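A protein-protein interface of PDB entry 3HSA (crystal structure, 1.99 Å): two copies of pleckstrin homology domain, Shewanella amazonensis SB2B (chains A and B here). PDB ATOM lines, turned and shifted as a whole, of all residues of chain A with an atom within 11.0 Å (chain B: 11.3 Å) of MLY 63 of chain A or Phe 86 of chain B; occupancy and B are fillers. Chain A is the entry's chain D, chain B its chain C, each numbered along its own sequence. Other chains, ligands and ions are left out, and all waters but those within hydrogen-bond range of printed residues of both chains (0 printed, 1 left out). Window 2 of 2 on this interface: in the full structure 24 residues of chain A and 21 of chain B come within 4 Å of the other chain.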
ATOM      1  N   GLU A  23     -24.472  20.978  26.889  1.00  0.00           N
ATOM      2  CA  GLU A  23     -23.947  21.466  25.617  1.00  0.00           C
ATOM      3  C   GLU A  23     -24.887  22.471  24.912  1.00  0.00           C
ATOM      4  O   GLU A  23     -24.441  23.499  24.409  1.00  0.00           O
ATOM      5  CB  GLU A  23     -23.665  20.296  24.678  1.00  0.00           C
ATOM      6  CG  GLU A  23     -23.112  20.749  23.332  1.00  0.00           C
ATOM      7  CD  GLU A  23     -22.758  19.626  22.366  1.00  0.00           C
ATOM      8  OE1 GLU A  23     -22.654  18.459  22.759  1.00  0.00           O
ATOM      9  OE2 GLU A  23     -22.590  19.938  21.176  1.00  0.00           O
ATOM     10  N   ILE A  55     -27.471  17.341  15.383  1.00  0.00           N
ATOM     11  CA  ILE A  55     -26.110  17.685  15.776  1.00  0.00           C
ATOM     12  C   ILE A  55     -25.140  16.773  15.026  1.00  0.00           C
ATOM     13  O   ILE A  55     -25.206  15.547  15.183  1.00  0.00           O
ATOM     14  CB  ILE A  55     -25.880  17.505  17.289  1.00  0.00           C
ATOM     15  CG1 ILE A  55     -26.873  18.358  18.093  1.00  0.00           C
ATOM     16  CG2 ILE A  55     -24.384  17.821  17.675  1.00  0.00           C
ATOM     17  CD1 ILE A  55     -26.806  18.146  19.593  1.00  0.00           C
ATOM     18  N   ASP A  56     -24.253  17.385  14.236  1.00  0.00           N
ATOM     19  CA  ASP A  56     -23.222  16.689  13.489  1.00  0.00           C
ATOM     20  C   ASP A  56     -21.835  17.214  13.881  1.00  0.00           C
ATOM     21  O   ASP A  56     -21.486  18.382  13.644  1.00  0.00           O
ATOM     22  CB  ASP A  56     -23.484  16.848  11.987  1.00  0.00           C
ATOM     23  CG  ASP A  56     -22.527  16.022  11.137  1.00  0.00           C
ATOM     24  OD1 ASP A  56     -21.646  15.340  11.702  1.00  0.00           O
ATOM     25  OD2 ASP A  56     -22.651  16.061   9.904  1.00  0.00           O
ATOM     26  N   MLY A  57     -21.045  16.375  14.537  1.00  0.00           N
ATOM     27  CA  MLY A  57     -19.705  16.769  14.978  1.00  0.00           C
ATOM     28  CB  MLY A  57     -19.491  16.414  16.460  1.00  0.00           C
ATOM     29  CG  MLY A  57     -20.282  17.259  17.449  1.00  0.00           C
ATOM     30  CD  MLY A  57     -20.368  16.597  18.837  1.00  0.00           C
ATOM     31  CE  MLY A  57     -20.836  17.584  19.936  1.00  0.00           C
ATOM     32  NZ  MLY A  57     -21.207  16.907  21.249  1.00  0.00           N
ATOM     33  CH1 MLY A  57     -22.414  16.045  21.105  1.00  0.00           C
ATOM     34  CH2 MLY A  57     -20.119  16.101  21.821  1.00  0.00           C
ATOM     35  C   MLY A  57     -18.772  15.978  14.115  1.00  0.00           C
ATOM     36  O   MLY A  57     -18.843  14.739  14.106  1.00  0.00           O
ATOM     37  N   GLN A  58     -17.933  16.649  13.342  1.00  0.00           N
ATOM     38  CA  GLN A  58     -17.167  15.915  12.328  1.00  0.00           C
ATOM     39  C   GLN A  58     -15.682  15.951  12.529  1.00  0.00           C
ATOM     40  O   GLN A  58     -15.175  16.748  13.285  1.00  0.00           O
ATOM     41  CB  GLN A  58     -17.521  16.408  10.913  1.00  0.00           C
ATOM     42  CG  GLN A  58     -18.780  15.702  10.327  1.00  0.00           C
ATOM     43  CD  GLN A  58     -18.721  14.147  10.421  1.00  0.00           C
ATOM     44  OE1 GLN A  58     -17.678  13.536  10.076  1.00  0.00           O
ATOM     45  NE2 GLN A  58     -19.822  13.510  10.910  1.00  0.00           N
ATOM     46  N   GLY A  59     -15.005  15.068  11.813  1.00  0.00           N
ATOM     47  CA  GLY A  59     -13.558  15.003  11.824  1.00  0.00           C
ATOM     48  C   GLY A  59     -13.101  14.066  12.918  1.00  0.00           C
ATOM     49  O   GLY A  59     -13.906  13.557  13.699  1.00  0.00           O
ATOM     50  N   VAL A  60     -11.811  13.805  12.931  1.00  0.00           N
ATOM     51  CA  VAL A  60     -11.187  13.021  13.983  1.00  0.00           C
ATOM     52  C   VAL A  60     -11.200  13.843  15.281  1.00  0.00           C
ATOM     53  O   VAL A  60     -11.363  13.296  16.359  1.00  0.00           O
ATOM     54  CB  VAL A  60      -9.726  12.627  13.592  1.00  0.00           C
ATOM     55  CG1 VAL A  60      -9.074  11.799  14.681  1.00  0.00           C
ATOM     56  CG2 VAL A  60      -9.707  11.865  12.232  1.00  0.00           C
ATOM     57  N   THR A  61     -11.036  15.159  15.167  1.00  0.00           N
ATOM     58  CA  THR A  61     -10.944  16.027  16.329  1.00  0.00           C
ATOM     59  C   THR A  61     -12.332  16.487  16.786  1.00  0.00           C
ATOM     60  O   THR A  61     -12.471  17.009  17.878  1.00  0.00           O
ATOM     61  CB  THR A  61     -10.063  17.256  16.024  1.00  0.00           C
ATOM     62  OG1 THR A  61     -10.577  17.921  14.867  1.00  0.00           O
ATOM     63  CG2 THR A  61      -8.608  16.847  15.766  1.00  0.00           C
ATOM     64  N   GLY A  62     -13.348  16.293  15.941  1.00  0.00           N
ATOM     65  CA  GLY A  62     -14.721  16.706  16.265  1.00  0.00           C
ATOM     66  C   GLY A  62     -14.900  18.211  16.421  1.00  0.00           C
ATOM     67  O   GLY A  62     -15.834  18.632  17.081  1.00  0.00           O
ATOM     68  N   MLY A  63     -14.028  19.010  15.808  1.00  0.00           N
ATOM     69  CA  MLY A  63     -14.071  20.480  15.910  1.00  0.00           C
ATOM     70  CB  MLY A  63     -12.761  21.107  15.437  1.00  0.00           C
ATOM     71  CG  MLY A  63     -11.561  20.797  16.281  1.00  0.00           C
ATOM     72  CD  MLY A  63     -10.291  20.952  15.469  1.00  0.00           C
ATOM     73  CE  MLY A  63     -10.066  22.341  14.905  1.00  0.00           C
ATOM     74  NZ  MLY A  63      -8.817  22.262  14.090  1.00  0.00           N
ATOM     75  C   MLY A  63     -15.143  21.109  15.050  1.00  0.00           C
ATOM     76  O   MLY A  63     -15.643  22.167  15.406  1.00  0.00           O
ATOM     77  N   MLY A  64     -15.421  20.522  13.885  1.00  0.00           N
ATOM     78  CA  MLY A  64     -16.448  21.053  12.977  1.00  0.00           C
ATOM     79  CB  MLY A  64     -16.187  20.610  11.545  1.00  0.00           C
ATOM     80  CG  MLY A  64     -16.964  21.403  10.499  1.00  0.00           C
ATOM     81  CD  MLY A  64     -16.520  21.071   9.080  1.00  0.00           C
ATOM     82  CE  MLY A  64     -17.071  22.094   8.080  1.00  0.00           C
ATOM     83  NZ  MLY A  64     -16.549  23.488   8.386  1.00  0.00           N
ATOM     84  C   MLY A  64     -17.838  20.578  13.444  1.00  0.00           C
ATOM     85  O   MLY A  64     -18.179  19.388  13.306  1.00  0.00           O
ATOM     86  N   VAL A  65     -18.629  21.502  13.991  1.00  0.00           N
ATOM     87  CA  VAL A  65     -19.922  21.153  14.573  1.00  0.00           C
ATOM     88  C   VAL A  65     -21.055  21.952  13.938  1.00  0.00           C
ATOM     89  O   VAL A  65     -20.901  23.151  13.733  1.00  0.00           O
ATOM     90  CB  VAL A  65     -19.906  21.381  16.089  1.00  0.00           C
ATOM     91  CG1 VAL A  65     -21.255  20.964  16.718  1.00  0.00           C
ATOM     92  CG2 VAL A  65     -18.718  20.582  16.711  1.00  0.00           C
ATOM     93  N   SER A  66     -22.142  21.286  13.561  1.00  0.00           N
ATOM     94  CA  SER A  66     -23.362  22.002  13.133  1.00  0.00           C
ATOM     95  C   SER A  66     -24.562  21.637  13.989  1.00  0.00           C
ATOM     96  O   SER A  66     -24.723  20.462  14.377  1.00  0.00           O
ATOM     97  CB  SER A  66     -23.678  21.722  11.669  1.00  0.00           C
ATOM     98  OG  SER A  66     -23.938  20.390  11.437  1.00  0.00           O
ATOM     99  N   TYR A  67     -25.393  22.640  14.272  1.00  0.00           N
ATOM    100  CA  TYR A  67     -26.659  22.433  14.935  1.00  0.00           C
ATOM    101  C   TYR A  67     -27.714  22.852  13.937  1.00  0.00           C
ATOM    102  O   TYR A  67     -27.824  24.023  13.634  1.00  0.00           O
ATOM    103  CB  TYR A  67     -26.826  23.281  16.209  1.00  0.00           C
ATOM    104  CG  TYR A  67     -25.830  23.020  17.301  1.00  0.00           C
ATOM    105  CD1 TYR A  67     -25.416  21.738  17.601  1.00  0.00           C
ATOM    106  CD2 TYR A  67     -25.347  24.054  18.090  1.00  0.00           C
ATOM    107  CE1 TYR A  67     -24.518  21.482  18.630  1.00  0.00           C
ATOM    108  CE2 TYR A  67     -24.423  23.804  19.139  1.00  0.00           C
ATOM    109  CZ  TYR A  67     -24.005  22.507  19.374  1.00  0.00           C
ATOM    110  OH  TYR A  67     -23.106  22.219  20.387  1.00  0.00           O
ATOM    111  N   VAL B  80     -26.564  26.700  12.539  1.00  0.00           N
ATOM    112  CA  VAL B  80     -25.317  27.379  12.794  1.00  0.00           C
ATOM    113  C   VAL B  80     -24.253  26.289  12.757  1.00  0.00           C
ATOM    114  O   VAL B  80     -24.424  25.224  13.367  1.00  0.00           O
ATOM    115  CB  VAL B  80     -25.318  28.142  14.126  1.00  0.00           C
ATOM    116  CG1 VAL B  80     -23.970  28.822  14.348  1.00  0.00           C
ATOM    117  CG2 VAL B  80     -26.423  29.210  14.114  1.00  0.00           C
ATOM    118  N   GLU B  81     -23.176  26.557  12.021  1.00  0.00           N
ATOM    119  CA  GLU B  81     -22.076  25.627  11.880  1.00  0.00           C
ATOM    120  C   GLU B  81     -20.758  26.372  12.079  1.00  0.00           C
ATOM    121  O   GLU B  81     -20.655  27.572  11.808  1.00  0.00           O
ATOM    122  CB  GLU B  81     -22.110  24.978  10.488  1.00  0.00           C
ATOM    123  CG  GLU B  81     -21.006  23.912  10.283  1.00  0.00           C
ATOM    124  CD  GLU B  81     -21.223  23.030   9.048  1.00  0.00           C
ATOM    125  OE1 GLU B  81     -21.661  23.566   7.995  1.00  0.00           O
ATOM    126  OE2 GLU B  81     -20.942  21.807   9.150  1.00  0.00           O
ATOM    127  N   THR B  82     -19.743  25.671  12.557  1.00  0.00           N
ATOM    128  CA  THR B  82     -18.425  26.277  12.663  1.00  0.00           C
ATOM    129  C   THR B  82     -17.842  26.459  11.240  1.00  0.00           C
ATOM    130  O   THR B  82     -18.207  25.752  10.286  1.00  0.00           O
ATOM    131  CB  THR B  82     -17.504  25.473  13.592  1.00  0.00           C
ATOM    132  OG1 THR B  82     -17.343  24.161  13.071  1.00  0.00           O
ATOM    133  CG2 THR B  82     -18.096  25.377  14.965  1.00  0.00           C
ATOM    134  N   ALA B  83     -16.988  27.462  11.092  1.00  0.00           N
ATOM    135  CA  ALA B  83     -16.406  27.810   9.798  1.00  0.00           C
ATOM    136  C   ALA B  83     -15.068  28.546   9.993  1.00  0.00           C
ATOM    137  O   ALA B  83     -14.653  28.855  11.122  1.00  0.00           O
ATOM    138  CB  ALA B  83     -17.386  28.678   8.976  1.00  0.00           C
ATOM    139  N   GLY B  84     -14.406  28.822   8.876  1.00  0.00           N
ATOM    140  CA  GLY B  84     -13.111  29.506   8.895  1.00  0.00           C
ATOM    141  C   GLY B  84     -12.009  28.544   9.289  1.00  0.00           C
ATOM    142  O   GLY B  84     -12.264  27.381   9.665  1.00  0.00           O
ATOM    143  N   THR B  85     -10.773  29.011   9.182  1.00  0.00           N
ATOM    144  CA  THR B  85      -9.628  28.197   9.555  1.00  0.00           C
ATOM    145  C   THR B  85      -9.741  27.751  11.023  1.00  0.00           C
ATOM    146  O   THR B  85     -10.113  28.554  11.880  1.00  0.00           O
ATOM    147  CB  THR B  85      -8.315  28.960   9.362  1.00  0.00           C
ATOM    148  OG1 THR B  85      -7.234  28.106   9.759  1.00  0.00           O
ATOM    149  CG2 THR B  85      -8.288  30.248  10.186  1.00  0.00           C
ATOM    150  N   PHE B  86      -9.460  26.474  11.303  1.00  0.00           N
ATOM    151  CA  PHE B  86      -9.504  25.953  12.685  1.00  0.00           C
ATOM    152  C   PHE B  86     -10.921  26.097  13.340  1.00  0.00           C
ATOM    153  O   PHE B  86     -11.060  26.085  14.568  1.00  0.00           O
ATOM    154  CB  PHE B  86      -8.401  26.661  13.497  1.00  0.00           C
ATOM    155  CG  PHE B  86      -8.006  25.973  14.782  1.00  0.00           C
ATOM    156  CD1 PHE B  86      -7.467  24.699  14.767  1.00  0.00           C
ATOM    157  CD2 PHE B  86      -8.092  26.651  16.000  1.00  0.00           C
ATOM    158  CE1 PHE B  86      -7.076  24.065  15.960  1.00  0.00           C
ATOM    159  CE2 PHE B  86      -7.694  26.041  17.199  1.00  0.00           C
ATOM    160  CZ  PHE B  86      -7.192  24.744  17.177  1.00  0.00           C
ATOM    161  N   ASP B  87     -11.964  26.231  12.507  1.00  0.00           N
ATOM    162  CA  ASP B  87     -13.360  26.279  12.970  1.00  0.00           C
ATOM    163  C   ASP B  87     -13.683  27.309  14.065  1.00  0.00           C
ATOM    164  O   ASP B  87     -14.537  27.092  14.908  1.00  0.00           O
ATOM    165  CB  ASP B  87     -13.782  24.863  13.367  1.00  0.00           C
ATOM    166  CG  ASP B  87     -14.023  24.002  12.169  1.00  0.00           C
ATOM    167  OD1 ASP B  87     -15.060  24.215  11.498  1.00  0.00           O
ATOM    168  OD2 ASP B  87     -13.194  23.112  11.892  1.00  0.00           O
ATOM    169  N   MET B  88     -13.027  28.463  13.997  1.00  0.00           N
ATOM    170  CA  MET B  88     -13.211  29.535  14.996  1.00  0.00           C
ATOM    171  C   MET B  88     -14.347  30.482  14.646  1.00  0.00           C
ATOM    172  O   MET B  88     -14.875  31.144  15.533  1.00  0.00           O
ATOM    173  CB  MET B  88     -11.925  30.356  15.157  1.00  0.00           C
ATOM    174  CG  MET B  88     -10.662  29.544  15.522  1.00  0.00           C
ATOM    175  SD  MET B  88     -10.546  28.972  17.405  1.00  0.00           S
ATOM    176  CE  MET B  88     -10.182  30.709  18.209  1.00  0.00           C
ATOM    177  N   ASP B  89     -14.689  30.607  13.363  1.00  0.00           N
ATOM    178  CA  ASP B  89     -15.853  31.439  12.983  1.00  0.00           C
ATOM    179  C   ASP B  89     -17.093  30.563  12.914  1.00  0.00           C
ATOM    180  O   ASP B  89     -17.016  29.355  13.155  1.00  0.00           O
ATOM    181  CB  ASP B  89     -15.626  32.134  11.641  1.00  0.00           C
ATOM    182  CG  ASP B  89     -14.424  33.069  11.666  1.00  0.00           C
ATOM    183  OD1 ASP B  89     -14.278  33.845  12.653  1.00  0.00           O
ATOM    184  OD2 ASP B  89     -13.656  33.031  10.671  1.00  0.00           O
ATOM    185  N   ALA B  90     -18.242  31.183  12.643  1.00  0.00           N
ATOM    186  CA  ALA B  90     -19.499  30.441  12.463  1.00  0.00           C
ATOM    187  C   ALA B  90     -20.196  30.911  11.209  1.00  0.00           C
ATOM    188  O   ALA B  90     -19.955  32.032  10.719  1.00  0.00           O
ATOM    189  CB  ALA B  90     -20.408  30.616  13.652  1.00  0.00           C
ATOM    190  N   GLU B  91     -21.057  30.043  10.699  1.00  0.00           N
ATOM    191  CA  GLU B  91     -21.888  30.332   9.562  1.00  0.00           C
ATOM    192  C   GLU B  91     -23.353  30.038   9.919  1.00  0.00           C
ATOM    193  O   GLU B  91     -23.666  28.957  10.417  1.00  0.00           O
ATOM    194  CB  GLU B  91     -21.437  29.483   8.385  1.00  0.00           C
ATOM    195  CG  GLU B  91     -22.110  29.800   7.106  1.00  0.00           C
ATOM    196  CD  GLU B  91     -21.366  29.246   5.908  1.00  0.00           C
ATOM    197  OE1 GLU B  91     -20.379  29.890   5.486  1.00  0.00           O
ATOM    198  OE2 GLU B  91     -21.791  28.197   5.384  1.00  0.00           O
ATOM    199  N   LEU B 107     -20.725  34.657  10.625  1.00  0.00           N
ATOM    200  CA  LEU B 107     -20.658  35.234  11.948  1.00  0.00           C
ATOM    201  C   LEU B 107     -19.195  35.053  12.365  1.00  0.00           C
ATOM    202  O   LEU B 107     -18.825  34.009  12.891  1.00  0.00           O
ATOM    203  CB  LEU B 107     -21.623  34.523  12.910  1.00  0.00           C
ATOM    204  CG  LEU B 107     -23.052  34.201  12.413  1.00  0.00           C
ATOM    205  CD1 LEU B 107     -23.832  33.454  13.488  1.00  0.00           C
ATOM    206  CD2 LEU B 107     -23.802  35.427  12.003  1.00  0.00           C
ATOM    207  N   ARG B 109     -15.682  35.267  14.489  1.00  0.00           N
ATOM    208  CA  ARG B 109     -15.494  35.195  15.950  1.00  0.00           C
ATOM    209  C   ARG B 109     -15.480  36.620  16.480  1.00  0.00           C
ATOM    210  O   ARG B 109     -14.890  37.498  15.862  1.00  0.00           O
ATOM    211  CB  ARG B 109     -14.218  34.464  16.398  1.00  0.00           C
ATOM    212  CG  ARG B 109     -14.277  34.111  17.905  1.00  0.00           C
ATOM    213  CD  ARG B 109     -13.234  33.105  18.348  1.00  0.00           C
ATOM    214  NE  ARG B 109     -11.936  33.756  18.476  1.00  0.00           N
ATOM    215  CZ  ARG B 109     -11.235  33.918  19.599  1.00  0.00           C
ATOM    216  NH1 ARG B 109     -11.634  33.435  20.781  1.00  0.00           N
ATOM    217  NH2 ARG B 109     -10.082  34.561  19.515  1.00  0.00           N
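MLY 63 of chain A touches Thr 82 of chain B. MLY 63 of chain A touches Phe 86 of chain B. Asp 87 of chain B touches MLY 63 of chain A. Asp 87 of chain B touches MLY 64 of chain A (OD1 to NZ, 3.5 Å). Glu 81 of chain B touches Val 65 of chain A. Ser 66 of chain A touches Val 80 of chain B. OE2 of Glu 81 of chain B touches CB of Ser 66 of chain A, at 3.7 Å.
O of Glu 81 of chain B sits at hydrogen-bond distance from N of Glu 91 of chain B (2.7 Å). OD1 of Asp 87 of chain B sits at hydrogen-bond distance from OG1 of Thr 82 of chain B. The side-chain carboxylate (OE2) of Glu 23 of chain A lies within hydrogen-bond range of the side-chain hydroxyl (OH) of Tyr 67 of chain A (2.5 Å). The backbone carbonyl oxygen (O) of Asp 56 of chain A lies within hydrogen-bond range of the backbone NH (N) of Ser 66 of chain A, at 3.0 Å. The backbone NH of Gln 58 of chain A is in hydrogen-bond range of O of MLY 64 of chain A (2.8 Å).
No residue of chain B comes within 4 Å of Gly 59 of chain A. No residue of chain B comes within 4 Å of Thr 61 of chain A. Printed residues of chain B within 4 Å of Val 65 of chain A: Glu 81 (3.3 Å) and Thr 82 (3.0 Å). Of the printed residues of chain B, Ser 66 of chain A touches Val 80 (3.4 Å) and Glu 81 (3.7 Å). Printed residues of chain B within 4 Å of Tyr 67 of chain A: Val 80 (2.9 Å). Printed residues of chain A within 4 Å of Val 80 of chain B: Ser 66 and Tyr 67. Printed residues of chain A within 4 Å of Glu 81 of chain B: Val 65 (3.3 Å) and Ser 66 (3.7 Å). No residue of chain A comes within 4 Å of Thr 85 of chain B. Printed residues of chain A within 4 Å of Asp 87 of chain B: MLY 63 and MLY 64. The nearest residue of chain B that does not touch MLY 63 of chain A is Thr 85 of chain B (6.4 Å). The nearest residue of chain A that does not touch Phe 86 of chain B is MLY 64 of chain A (7.1 Å).
O of Val 80 of chain B lies within hydrogen-bond range of N of Tyr 67 of chain A (2.9 Å). The backbone carbonyl oxygen (O) of Thr 82 of chain B lies close to NZ of MLY 64 of chain A (3.4 Å). The backbone NH (N) of Thr 82 of chain B sits at hydrogen-bond distance from the backbone carbonyl oxygen (O) of Val 65 of chain A.
Of the 14 printed residues of chain A, 5 touch a printed residue of chain B. Of the 14 printed residues of chain B, 5 touch a printed residue of chain A. Hydrophobic or aromatic side chains of chain B that line the printed part of chain A: Phe 86. Among the printed residues, no Asp or Glu carboxylate lies within 4 Å of a Lys or Arg side-chain nitrogen of the other chain.
No position is printed for both chains. Of the 10 pairs that touch across the chains among the printed residues, none has its exchanged pair printed and touching as well.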
